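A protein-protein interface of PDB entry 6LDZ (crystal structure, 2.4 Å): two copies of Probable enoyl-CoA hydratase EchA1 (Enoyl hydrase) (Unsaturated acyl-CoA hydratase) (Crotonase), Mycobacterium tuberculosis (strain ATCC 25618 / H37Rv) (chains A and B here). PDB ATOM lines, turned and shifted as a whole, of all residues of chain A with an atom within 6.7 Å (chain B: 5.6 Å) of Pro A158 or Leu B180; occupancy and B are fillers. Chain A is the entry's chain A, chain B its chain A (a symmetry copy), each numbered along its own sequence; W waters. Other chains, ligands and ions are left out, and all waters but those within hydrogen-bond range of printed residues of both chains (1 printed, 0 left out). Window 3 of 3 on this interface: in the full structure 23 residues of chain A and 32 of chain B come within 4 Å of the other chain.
Among the printed residues, pairs that only touch across the chains: Pro A158 with Arg B156, Pro A158 with Leu B180, Pro A158 with Gly B181, Tyr A159 with Arg B156, Ala A160 with Arg B156, Ala A160 with Gly B181 and Ile A161 with Gly B181.
Printed residues of chain B within 4 Å of Pro A158: Arg B156, Leu B180 and Gly B181.
Leu B180 touches one residue of chain A.
Printed residues of chain B within 4 Å of Tyr A159: Arg B156.
Printed residues of chain B within 4 Å of Ala A160: Arg B156 (3.97 Å) and Gly B181 (3.8 Å).
Of the printed residues of chain A, Arg B156 touches Pro A158, Tyr A159 and Ala A160.
Of the printed residues of chain A, Gly B181 touches Pro A158, Ala A160 and Ile A161.
Printed residues of chain B within 4 Å of Ile A161: Gly B181.
His B178 touches none of the printed residues of chain A.
The nearest printed residue of chain B that does not touch Pro A158 is Leu B182 (5.1 Å).
The nearest residue of chain A that does not touch Leu B180 is Leu A180 (6.0 Å).
The nearest printed residue of chain B that does not touch Tyr A159 is Gly B181 (5.4 Å).
Of the 14 printed residues of chain A, 4 touch a printed residue of chain B.
Hydrophobic or aromatic side chains of chain A that line the printed part of chain B: Pro A158, Tyr A159, Ala A160 and Ile A161.
Among the printed residues, 7 pairs touch across the chains.
Pro A158 touches Arg B156, but with the chains exchanged Arg A156 does not touch Pro B158 (10.0 Å).
Pro A158 touches Leu B180, but with the chains exchanged Leu A180 does not touch Pro B158 (8.4 Å).
Pro A158 touches Gly B181, but with the chains exchanged Gly A181 does not touch Pro B158 (9.7 Å).
Ile A161 touches Gly B181, but with the chains exchanged Gly A181 does not touch Ile B161 (13.6 Å).
Of the 7 pairs that touch across the chains among the printed residues, none has its exchanged pair printed and touching as well.
Water W1 lies within hydrogen-bond range of the backbone carbonyl oxygen of Arg B156, the backbone NH of Ala A160, the backbone carbonyl oxygen of Gly B181 and the backbone NH of Tyr A159.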
ATOM      1  N   LEU A 153     -35.993 -22.872 -12.509  1.00  0.00           N
ATOM      2  CA  LEU A 153     -34.777 -23.344 -11.844  1.00  0.00           C
ATOM      3  C   LEU A 153     -33.928 -24.239 -12.742  1.00  0.00           C
ATOM      4  O   LEU A 153     -32.712 -23.996 -12.833  1.00  0.00           O
ATOM      5  CB  LEU A 153     -35.150 -24.045 -10.527  1.00  0.00           C
ATOM      6  CG  LEU A 153     -34.056 -24.300  -9.478  1.00  0.00           C
ATOM      7  CD1 LEU A 153     -33.266 -23.028  -9.127  1.00  0.00           C
ATOM      8  CD2 LEU A 153     -34.626 -24.969  -8.212  1.00  0.00           C
ATOM      9  N   PRO A 154     -34.486 -25.229 -13.460  1.00  0.00           N
ATOM     10  CA  PRO A 154     -33.648 -26.034 -14.372  1.00  0.00           C
ATOM     11  C   PRO A 154     -33.027 -25.241 -15.501  1.00  0.00           C
ATOM     12  O   PRO A 154     -32.090 -25.739 -16.135  1.00  0.00           O
ATOM     13  CB  PRO A 154     -34.617 -27.095 -14.920  1.00  0.00           C
ATOM     14  CG  PRO A 154     -35.730 -27.136 -13.963  1.00  0.00           C
ATOM     15  CD  PRO A 154     -35.871 -25.743 -13.410  1.00  0.00           C
ATOM     16  N   GLU A 155     -33.525 -24.040 -15.792  1.00  0.00           N
ATOM     17  CA  GLU A 155     -32.895 -23.160 -16.764  1.00  0.00           C
ATOM     18  C   GLU A 155     -31.953 -22.147 -16.127  1.00  0.00           C
ATOM     19  O   GLU A 155     -31.306 -21.380 -16.854  1.00  0.00           O
ATOM     20  CB  GLU A 155     -33.960 -22.414 -17.561  1.00  0.00           C
ATOM     21  CG  GLU A 155     -35.133 -23.261 -17.969  1.00  0.00           C
ATOM     22  CD  GLU A 155     -36.092 -22.502 -18.855  1.00  0.00           C
ATOM     23  OE1 GLU A 155     -36.138 -21.254 -18.759  1.00  0.00           O
ATOM     24  OE2 GLU A 155     -36.791 -23.153 -19.656  1.00  0.00           O
ATOM     25  N   ARG A 156     -31.864 -22.121 -14.798  1.00  0.00           N
ATOM     26  CA  ARG A 156     -31.020 -21.158 -14.107  1.00  0.00           C
ATOM     27  C   ARG A 156     -29.790 -21.780 -13.466  1.00  0.00           C
ATOM     28  O   ARG A 156     -28.752 -21.120 -13.401  1.00  0.00           O
ATOM     29  CB  ARG A 156     -31.831 -20.405 -13.041  1.00  0.00           C
ATOM     30  CG  ARG A 156     -32.763 -19.356 -13.635  1.00  0.00           C
ATOM     31  CD  ARG A 156     -32.030 -18.036 -13.916  1.00  0.00           C
ATOM     32  NE  ARG A 156     -32.233 -17.039 -12.851  1.00  0.00           N
ATOM     33  CZ  ARG A 156     -33.305 -16.240 -12.757  1.00  0.00           C
ATOM     34  NH1 ARG A 156     -33.407 -15.362 -11.756  1.00  0.00           N
ATOM     35  NH2 ARG A 156     -34.281 -16.318 -13.665  1.00  0.00           N
ATOM     36  N   ILE A 157     -29.884 -23.024 -12.994  1.00  0.00           N
ATOM     37  CA  ILE A 157     -28.766 -23.761 -12.393  1.00  0.00           C
ATOM     38  C   ILE A 157     -28.687 -25.121 -13.078  1.00  0.00           C
ATOM     39  O   ILE A 157     -29.630 -25.485 -13.799  1.00  0.00           O
ATOM     40  CB  ILE A 157     -28.948 -23.891 -10.870  1.00  0.00           C
ATOM     41  CG1 ILE A 157     -30.137 -24.812 -10.553  1.00  0.00           C
ATOM     42  CG2 ILE A 157     -29.140 -22.514 -10.260  1.00  0.00           C
ATOM     43  CD1 ILE A 157     -30.287 -25.177  -9.072  1.00  0.00           C
ATOM     44  N   PRO A 158     -27.613 -25.897 -12.922  1.00  0.00           N
ATOM     45  CA  PRO A 158     -27.572 -27.211 -13.582  1.00  0.00           C
ATOM     46  C   PRO A 158     -28.820 -28.035 -13.280  1.00  0.00           C
ATOM     47  O   PRO A 158     -29.327 -28.044 -12.156  1.00  0.00           O
ATOM     48  CB  PRO A 158     -26.311 -27.857 -13.003  1.00  0.00           C
ATOM     49  CG  PRO A 158     -25.413 -26.684 -12.705  1.00  0.00           C
ATOM     50  CD  PRO A 158     -26.321 -25.558 -12.288  1.00  0.00           C
ATOM     51  N   TYR A 159     -29.322 -28.703 -14.326  1.00  0.00           N
ATOM     52  CA  TYR A 159     -30.569 -29.472 -14.280  1.00  0.00           C
ATOM     53  C   TYR A 159     -30.616 -30.447 -13.101  1.00  0.00           C
ATOM     54  O   TYR A 159     -31.633 -30.546 -12.403  1.00  0.00           O
ATOM     55  CB  TYR A 159     -30.736 -30.225 -15.613  1.00  0.00           C
ATOM     56  CG  TYR A 159     -31.899 -31.207 -15.680  1.00  0.00           C
ATOM     57  CD1 TYR A 159     -33.142 -30.803 -16.141  1.00  0.00           C
ATOM     58  CD2 TYR A 159     -31.740 -32.544 -15.303  1.00  0.00           C
ATOM     59  CE1 TYR A 159     -34.212 -31.706 -16.213  1.00  0.00           C
ATOM     60  CE2 TYR A 159     -32.794 -33.449 -15.375  1.00  0.00           C
ATOM     61  CZ  TYR A 159     -34.029 -33.023 -15.824  1.00  0.00           C
ATOM     62  OH  TYR A 159     -35.084 -33.913 -15.884  1.00  0.00           O
ATOM     63  N   ALA A 160     -29.539 -31.202 -12.878  1.00  0.00           N
ATOM     64  CA  ALA A 160     -29.571 -32.190 -11.801  1.00  0.00           C
ATOM     65  C   ALA A 160     -29.712 -31.516 -10.437  1.00  0.00           C
ATOM     66  O   ALA A 160     -30.436 -32.016  -9.562  1.00  0.00           O
ATOM     67  CB  ALA A 160     -28.329 -33.083 -11.848  1.00  0.00           C
ATOM     68  N   ILE A 161     -29.058 -30.363 -10.240  1.00  0.00           N
ATOM     69  CA  ILE A 161     -29.179 -29.657  -8.960  1.00  0.00           C
ATOM     70  C   ILE A 161     -30.608 -29.136  -8.763  1.00  0.00           C
ATOM     71  O   ILE A 161     -31.188 -29.261  -7.676  1.00  0.00           O
ATOM     72  CB  ILE A 161     -28.145 -28.515  -8.859  1.00  0.00           C
ATOM     73  CG1 ILE A 161     -26.750 -28.970  -9.330  1.00  0.00           C
ATOM     74  CG2 ILE A 161     -28.100 -27.984  -7.417  1.00  0.00           C
ATOM     75  CD1 ILE A 161     -26.265 -30.249  -8.673  1.00  0.00           C
ATOM     76  N   ALA A 162     -31.179 -28.510  -9.799  1.00  0.00           N
ATOM     77  CA  ALA A 162     -32.576 -28.097  -9.736  1.00  0.00           C
ATOM     78  C   ALA A 162     -33.466 -29.281  -9.384  1.00  0.00           C
ATOM     79  O   ALA A 162     -34.366 -29.171  -8.536  1.00  0.00           O
ATOM     80  CB  ALA A 162     -33.004 -27.485 -11.075  1.00  0.00           C
ATOM     81  N   MET A 163     -33.201 -30.438 -10.002  1.00  0.00           N
ATOM     82  CA  MET A 163     -34.014 -31.616  -9.727  1.00  0.00           C
ATOM     83  C   MET A 163     -33.866 -32.043  -8.276  1.00  0.00           C
ATOM     84  O   MET A 163     -34.865 -32.342  -7.602  1.00  0.00           O
ATOM     85  CB  MET A 163     -33.632 -32.755 -10.679  1.00  0.00           C
ATOM     86  CG  MET A 163     -34.278 -34.051 -10.335  1.00  0.00           C
ATOM     87  SD  MET A 163     -35.972 -34.143 -10.975  1.00  0.00           S
ATOM     88  CE  MET A 163     -35.662 -34.215 -12.771  1.00  0.00           C
ATOM     89  N   GLU A 179     -22.060 -20.079  -6.742  1.00  0.00           N
ATOM     90  CA  GLU A 179     -21.253 -21.003  -7.537  1.00  0.00           C
ATOM     91  C   GLU A 179     -22.044 -21.596  -8.707  1.00  0.00           C
ATOM     92  O   GLU A 179     -21.492 -21.789  -9.792  1.00  0.00           O
ATOM     93  CB  GLU A 179     -20.692 -22.116  -6.644  1.00  0.00           C
ATOM     94  CG  GLU A 179     -19.854 -21.604  -5.452  1.00  0.00           C
ATOM     95  CD  GLU A 179     -19.545 -22.689  -4.421  1.00  0.00           C
ATOM     96  OE1 GLU A 179     -20.293 -23.689  -4.370  1.00  0.00           O
ATOM     97  OE2 GLU A 179     -18.558 -22.543  -3.658  1.00  0.00           O
ATOM     98  N   LEU A 180     -23.338 -21.853  -8.528  1.00  0.00           N
ATOM     99  CA  LEU A 180     -24.132 -22.462  -9.587  1.00  0.00           C
ATOM    100  C   LEU A 180     -24.646 -21.461 -10.618  1.00  0.00           C
ATOM    101  O   LEU A 180     -25.282 -21.874 -11.593  1.00  0.00           O
ATOM    102  CB  LEU A 180     -25.317 -23.222  -8.971  1.00  0.00           C
ATOM    103  CG  LEU A 180     -24.905 -24.417  -8.099  1.00  0.00           C
ATOM    104  CD1 LEU A 180     -26.096 -24.990  -7.353  1.00  0.00           C
ATOM    105  CD2 LEU A 180     -24.224 -25.483  -8.941  1.00  0.00           C
ATOM    106  N   GLY A 181     -24.411 -20.165 -10.425  1.00  0.00           N
ATOM    107  CA  GLY A 181     -24.862 -19.174 -11.369  1.00  0.00           C
ATOM    108  C   GLY A 181     -26.245 -18.613 -11.111  1.00  0.00           C
ATOM    109  O   GLY A 181     -26.716 -17.791 -11.914  1.00  0.00           O
ATOM    110  N   ARG B 156     -26.897 -30.883 -19.206  1.00  0.00           N
ATOM    111  CA  ARG B 156     -26.539 -31.175 -17.826  1.00  0.00           C
ATOM    112  C   ARG B 156     -25.324 -30.403 -17.339  1.00  0.00           C
ATOM    113  O   ARG B 156     -25.266 -30.066 -16.155  1.00  0.00           O
ATOM    114  CB  ARG B 156     -26.300 -32.681 -17.642  1.00  0.00           C
ATOM    115  CG  ARG B 156     -27.591 -33.489 -17.614  1.00  0.00           C
ATOM    116  CD  ARG B 156     -28.234 -33.488 -16.219  1.00  0.00           C
ATOM    117  NE  ARG B 156     -27.921 -34.706 -15.453  1.00  0.00           N
ATOM    118  CZ  ARG B 156     -28.576 -35.868 -15.580  1.00  0.00           C
ATOM    119  NH1 ARG B 156     -28.226 -36.925 -14.842  1.00  0.00           N
ATOM    120  NH2 ARG B 156     -29.585 -35.979 -16.447  1.00  0.00           N
ATOM    121  N   ILE B 157     -24.361 -30.119 -18.217  1.00  0.00           N
ATOM    122  CA  ILE B 157     -23.157 -29.343 -17.894  1.00  0.00           C
ATOM    123  C   ILE B 157     -23.023 -28.242 -18.941  1.00  0.00           C
ATOM    124  O   ILE B 157     -23.729 -28.294 -19.960  1.00  0.00           O
ATOM    125  CB  ILE B 157     -21.915 -30.250 -17.846  1.00  0.00           C
ATOM    126  CG1 ILE B 157     -21.583 -30.773 -19.254  1.00  0.00           C
ATOM    127  CG2 ILE B 157     -22.155 -31.394 -16.877  1.00  0.00           C
ATOM    128  CD1 ILE B 157     -20.249 -31.520 -19.362  1.00  0.00           C
ATOM    129  N   PRO B 158     -22.175 -27.229 -18.752  1.00  0.00           N
ATOM    130  CA  PRO B 158     -22.055 -26.189 -19.787  1.00  0.00           C
ATOM    131  C   PRO B 158     -21.802 -26.791 -21.166  1.00  0.00           C
ATOM    132  O   PRO B 158     -21.045 -27.753 -21.318  1.00  0.00           O
ATOM    133  CB  PRO B 158     -20.868 -25.350 -19.307  1.00  0.00           C
ATOM    134  CG  PRO B 158     -20.915 -25.490 -17.806  1.00  0.00           C
ATOM    135  CD  PRO B 158     -21.416 -26.882 -17.532  1.00  0.00           C
ATOM    136  N   ILE B 161     -18.268 -27.504 -22.479  1.00  0.00           N
ATOM    137  CA  ILE B 161     -17.613 -28.644 -21.830  1.00  0.00           C
ATOM    138  C   ILE B 161     -18.161 -29.967 -22.378  1.00  0.00           C
ATOM    139  O   ILE B 161     -17.401 -30.900 -22.670  1.00  0.00           O
ATOM    140  CB  ILE B 161     -17.762 -28.567 -20.295  1.00  0.00           C
ATOM    141  CG1 ILE B 161     -17.480 -27.147 -19.768  1.00  0.00           C
ATOM    142  CG2 ILE B 161     -16.837 -29.601 -19.633  1.00  0.00           C
ATOM    143  CD1 ILE B 161     -16.165 -26.562 -20.252  1.00  0.00           C
ATOM    144  N   LEU B 172     -13.912 -37.138 -17.621  1.00  0.00           N
ATOM    145  CA  LEU B 172     -14.377 -36.061 -16.755  1.00  0.00           C
ATOM    146  C   LEU B 172     -14.280 -36.529 -15.308  1.00  0.00           C
ATOM    147  O   LEU B 172     -15.124 -37.318 -14.853  1.00  0.00           O
ATOM    148  CB  LEU B 172     -15.819 -35.675 -17.098  1.00  0.00           C
ATOM    149  CG  LEU B 172     -16.569 -34.746 -16.136  1.00  0.00           C
ATOM    150  CD1 LEU B 172     -15.928 -33.367 -16.137  1.00  0.00           C
ATOM    151  CD2 LEU B 172     -18.033 -34.664 -16.531  1.00  0.00           C
ATOM    152  N   GLU B 175     -14.734 -34.810  -9.370  1.00  0.00           N
ATOM    153  CA  GLU B 175     -14.637 -33.497  -8.729  1.00  0.00           C
ATOM    154  C   GLU B 175     -15.030 -32.378  -9.696  1.00  0.00           C
ATOM    155  O   GLU B 175     -15.762 -31.449  -9.328  1.00  0.00           O
ATOM    156  CB  GLU B 175     -13.225 -33.266  -8.192  1.00  0.00           C
ATOM    157  CG  GLU B 175     -12.762 -34.236  -7.113  1.00  0.00           C
ATOM    158  CD  GLU B 175     -11.639 -33.645  -6.278  1.00  0.00           C
ATOM    159  OE1 GLU B 175     -10.608 -33.292  -6.892  1.00  0.00           O
ATOM    160  OE2 GLU B 175     -11.769 -33.545  -5.031  1.00  0.00           O
ATOM    161  N   ARG B 176     -14.531 -32.441 -10.933  1.00  0.00           N
ATOM    162  CA  ARG B 176     -14.916 -31.468 -11.950  1.00  0.00           C
ATOM    163  C   ARG B 176     -16.398 -31.595 -12.293  1.00  0.00           C
ATOM    164  O   ARG B 176     -17.103 -30.588 -12.436  1.00  0.00           O
ATOM    165  CB  ARG B 176     -14.052 -31.653 -13.203  1.00  0.00           C
ATOM    166  CG  ARG B 176     -14.357 -30.672 -14.338  1.00  0.00           C
ATOM    167  CD  ARG B 176     -13.432 -29.483 -14.308  1.00  0.00           C
ATOM    168  NE  ARG B 176     -13.786 -28.452 -15.280  1.00  0.00           N
ATOM    169  CZ  ARG B 176     -13.500 -28.514 -16.582  1.00  0.00           C
ATOM    170  NH1 ARG B 176     -13.855 -27.520 -17.386  1.00  0.00           N
ATOM    171  NH2 ARG B 176     -12.863 -29.563 -17.091  1.00  0.00           N
ATOM    172  N   ALA B 177     -16.887 -32.834 -12.431  1.00  0.00           N
ATOM    173  CA  ALA B 177     -18.306 -33.053 -12.706  1.00  0.00           C
ATOM    174  C   ALA B 177     -19.181 -32.501 -11.590  1.00  0.00           C
ATOM    175  O   ALA B 177     -20.294 -32.024 -11.853  1.00  0.00           O
ATOM    176  CB  ALA B 177     -18.586 -34.545 -12.909  1.00  0.00           C
ATOM    177  N   HIS B 178     -18.704 -32.560 -10.337  1.00  0.00           N
ATOM    178  CA  HIS B 178     -19.439 -31.894  -9.266  1.00  0.00           C
ATOM    179  C   HIS B 178     -19.412 -30.374  -9.444  1.00  0.00           C
ATOM    180  O   HIS B 178     -20.447 -29.715  -9.305  1.00  0.00           O
ATOM    181  CB  HIS B 178     -18.891 -32.294  -7.895  1.00  0.00           C
ATOM    182  CG  HIS B 178     -19.630 -31.660  -6.757  1.00  0.00           C
ATOM    183  ND1 HIS B 178     -20.947 -31.961  -6.462  1.00  0.00           N
ATOM    184  CD2 HIS B 178     -19.246 -30.730  -5.850  1.00  0.00           C
ATOM    185  CE1 HIS B 178     -21.339 -31.243  -5.423  1.00  0.00           C
ATOM    186  NE2 HIS B 178     -20.328 -30.490  -5.033  1.00  0.00           N
ATOM    187  N   GLU B 179     -18.245 -29.802  -9.764  1.00  0.00           N
ATOM    188  CA  GLU B 179     -18.182 -28.366 -10.026  1.00  0.00           C
ATOM    189  C   GLU B 179     -19.093 -27.953 -11.186  1.00  0.00           C
ATOM    190  O   GLU B 179     -19.704 -26.884 -11.142  1.00  0.00           O
ATOM    191  CB  GLU B 179     -16.734 -27.942 -10.297  1.00  0.00           C
ATOM    192  CG  GLU B 179     -15.751 -28.296  -9.160  1.00  0.00           C
ATOM    193  CD  GLU B 179     -14.284 -28.132  -9.556  1.00  0.00           C
ATOM    194  OE1 GLU B 179     -13.990 -28.171 -10.771  1.00  0.00           O
ATOM    195  OE2 GLU B 179     -13.423 -27.967  -8.657  1.00  0.00           O
ATOM    196  N   LEU B 180     -19.232 -28.794 -12.208  1.00  0.00           N
ATOM    197  CA  LEU B 180     -20.045 -28.438 -13.364  1.00  0.00           C
ATOM    198  C   LEU B 180     -21.536 -28.699 -13.165  1.00  0.00           C
ATOM    199  O   LEU B 180     -22.327 -28.379 -14.058  1.00  0.00           O
ATOM    200  CB  LEU B 180     -19.549 -29.203 -14.600  1.00  0.00           C
ATOM    201  CG  LEU B 180     -18.125 -28.827 -15.034  1.00  0.00           C
ATOM    202  CD1 LEU B 180     -17.616 -29.761 -16.117  1.00  0.00           C
ATOM    203  CD2 LEU B 180     -18.070 -27.379 -15.491  1.00  0.00           C
ATOM    204  N   GLY B 181     -21.939 -29.283 -12.040  1.00  0.00           N
ATOM    205  CA  GLY B 181     -23.335 -29.545 -11.790  1.00  0.00           C
ATOM    206  C   GLY B 181     -23.838 -30.890 -12.269  1.00  0.00           C
ATOM    207  O   GLY B 181     -25.042 -31.162 -12.131  1.00  0.00           O
ATOM    208  N   LEU B 182     -22.966 -31.731 -12.840  1.00  0.00           N
ATOM    209  CA  LEU B 182     -23.371 -33.079 -13.240  1.00  0.00           C
ATOM    210  C   LEU B 182     -23.579 -33.984 -12.025  1.00  0.00           C
ATOM    211  O   LEU B 182     -24.554 -34.740 -11.967  1.00  0.00           O
ATOM    212  CB  LEU B 182     -22.319 -33.684 -14.173  1.00  0.00           C
ATOM    213  CG  LEU B 182     -22.577 -35.094 -14.705  1.00  0.00           C
ATOM    214  CD1 LEU B 182     -23.830 -35.138 -15.597  1.00  0.00           C
ATOM    215  CD2 LEU B 182     -21.362 -35.562 -15.472  1.00  0.00           C
HETATM  216  O   HOH W   1     -27.016 -31.319 -14.285  1.00  0.00           O
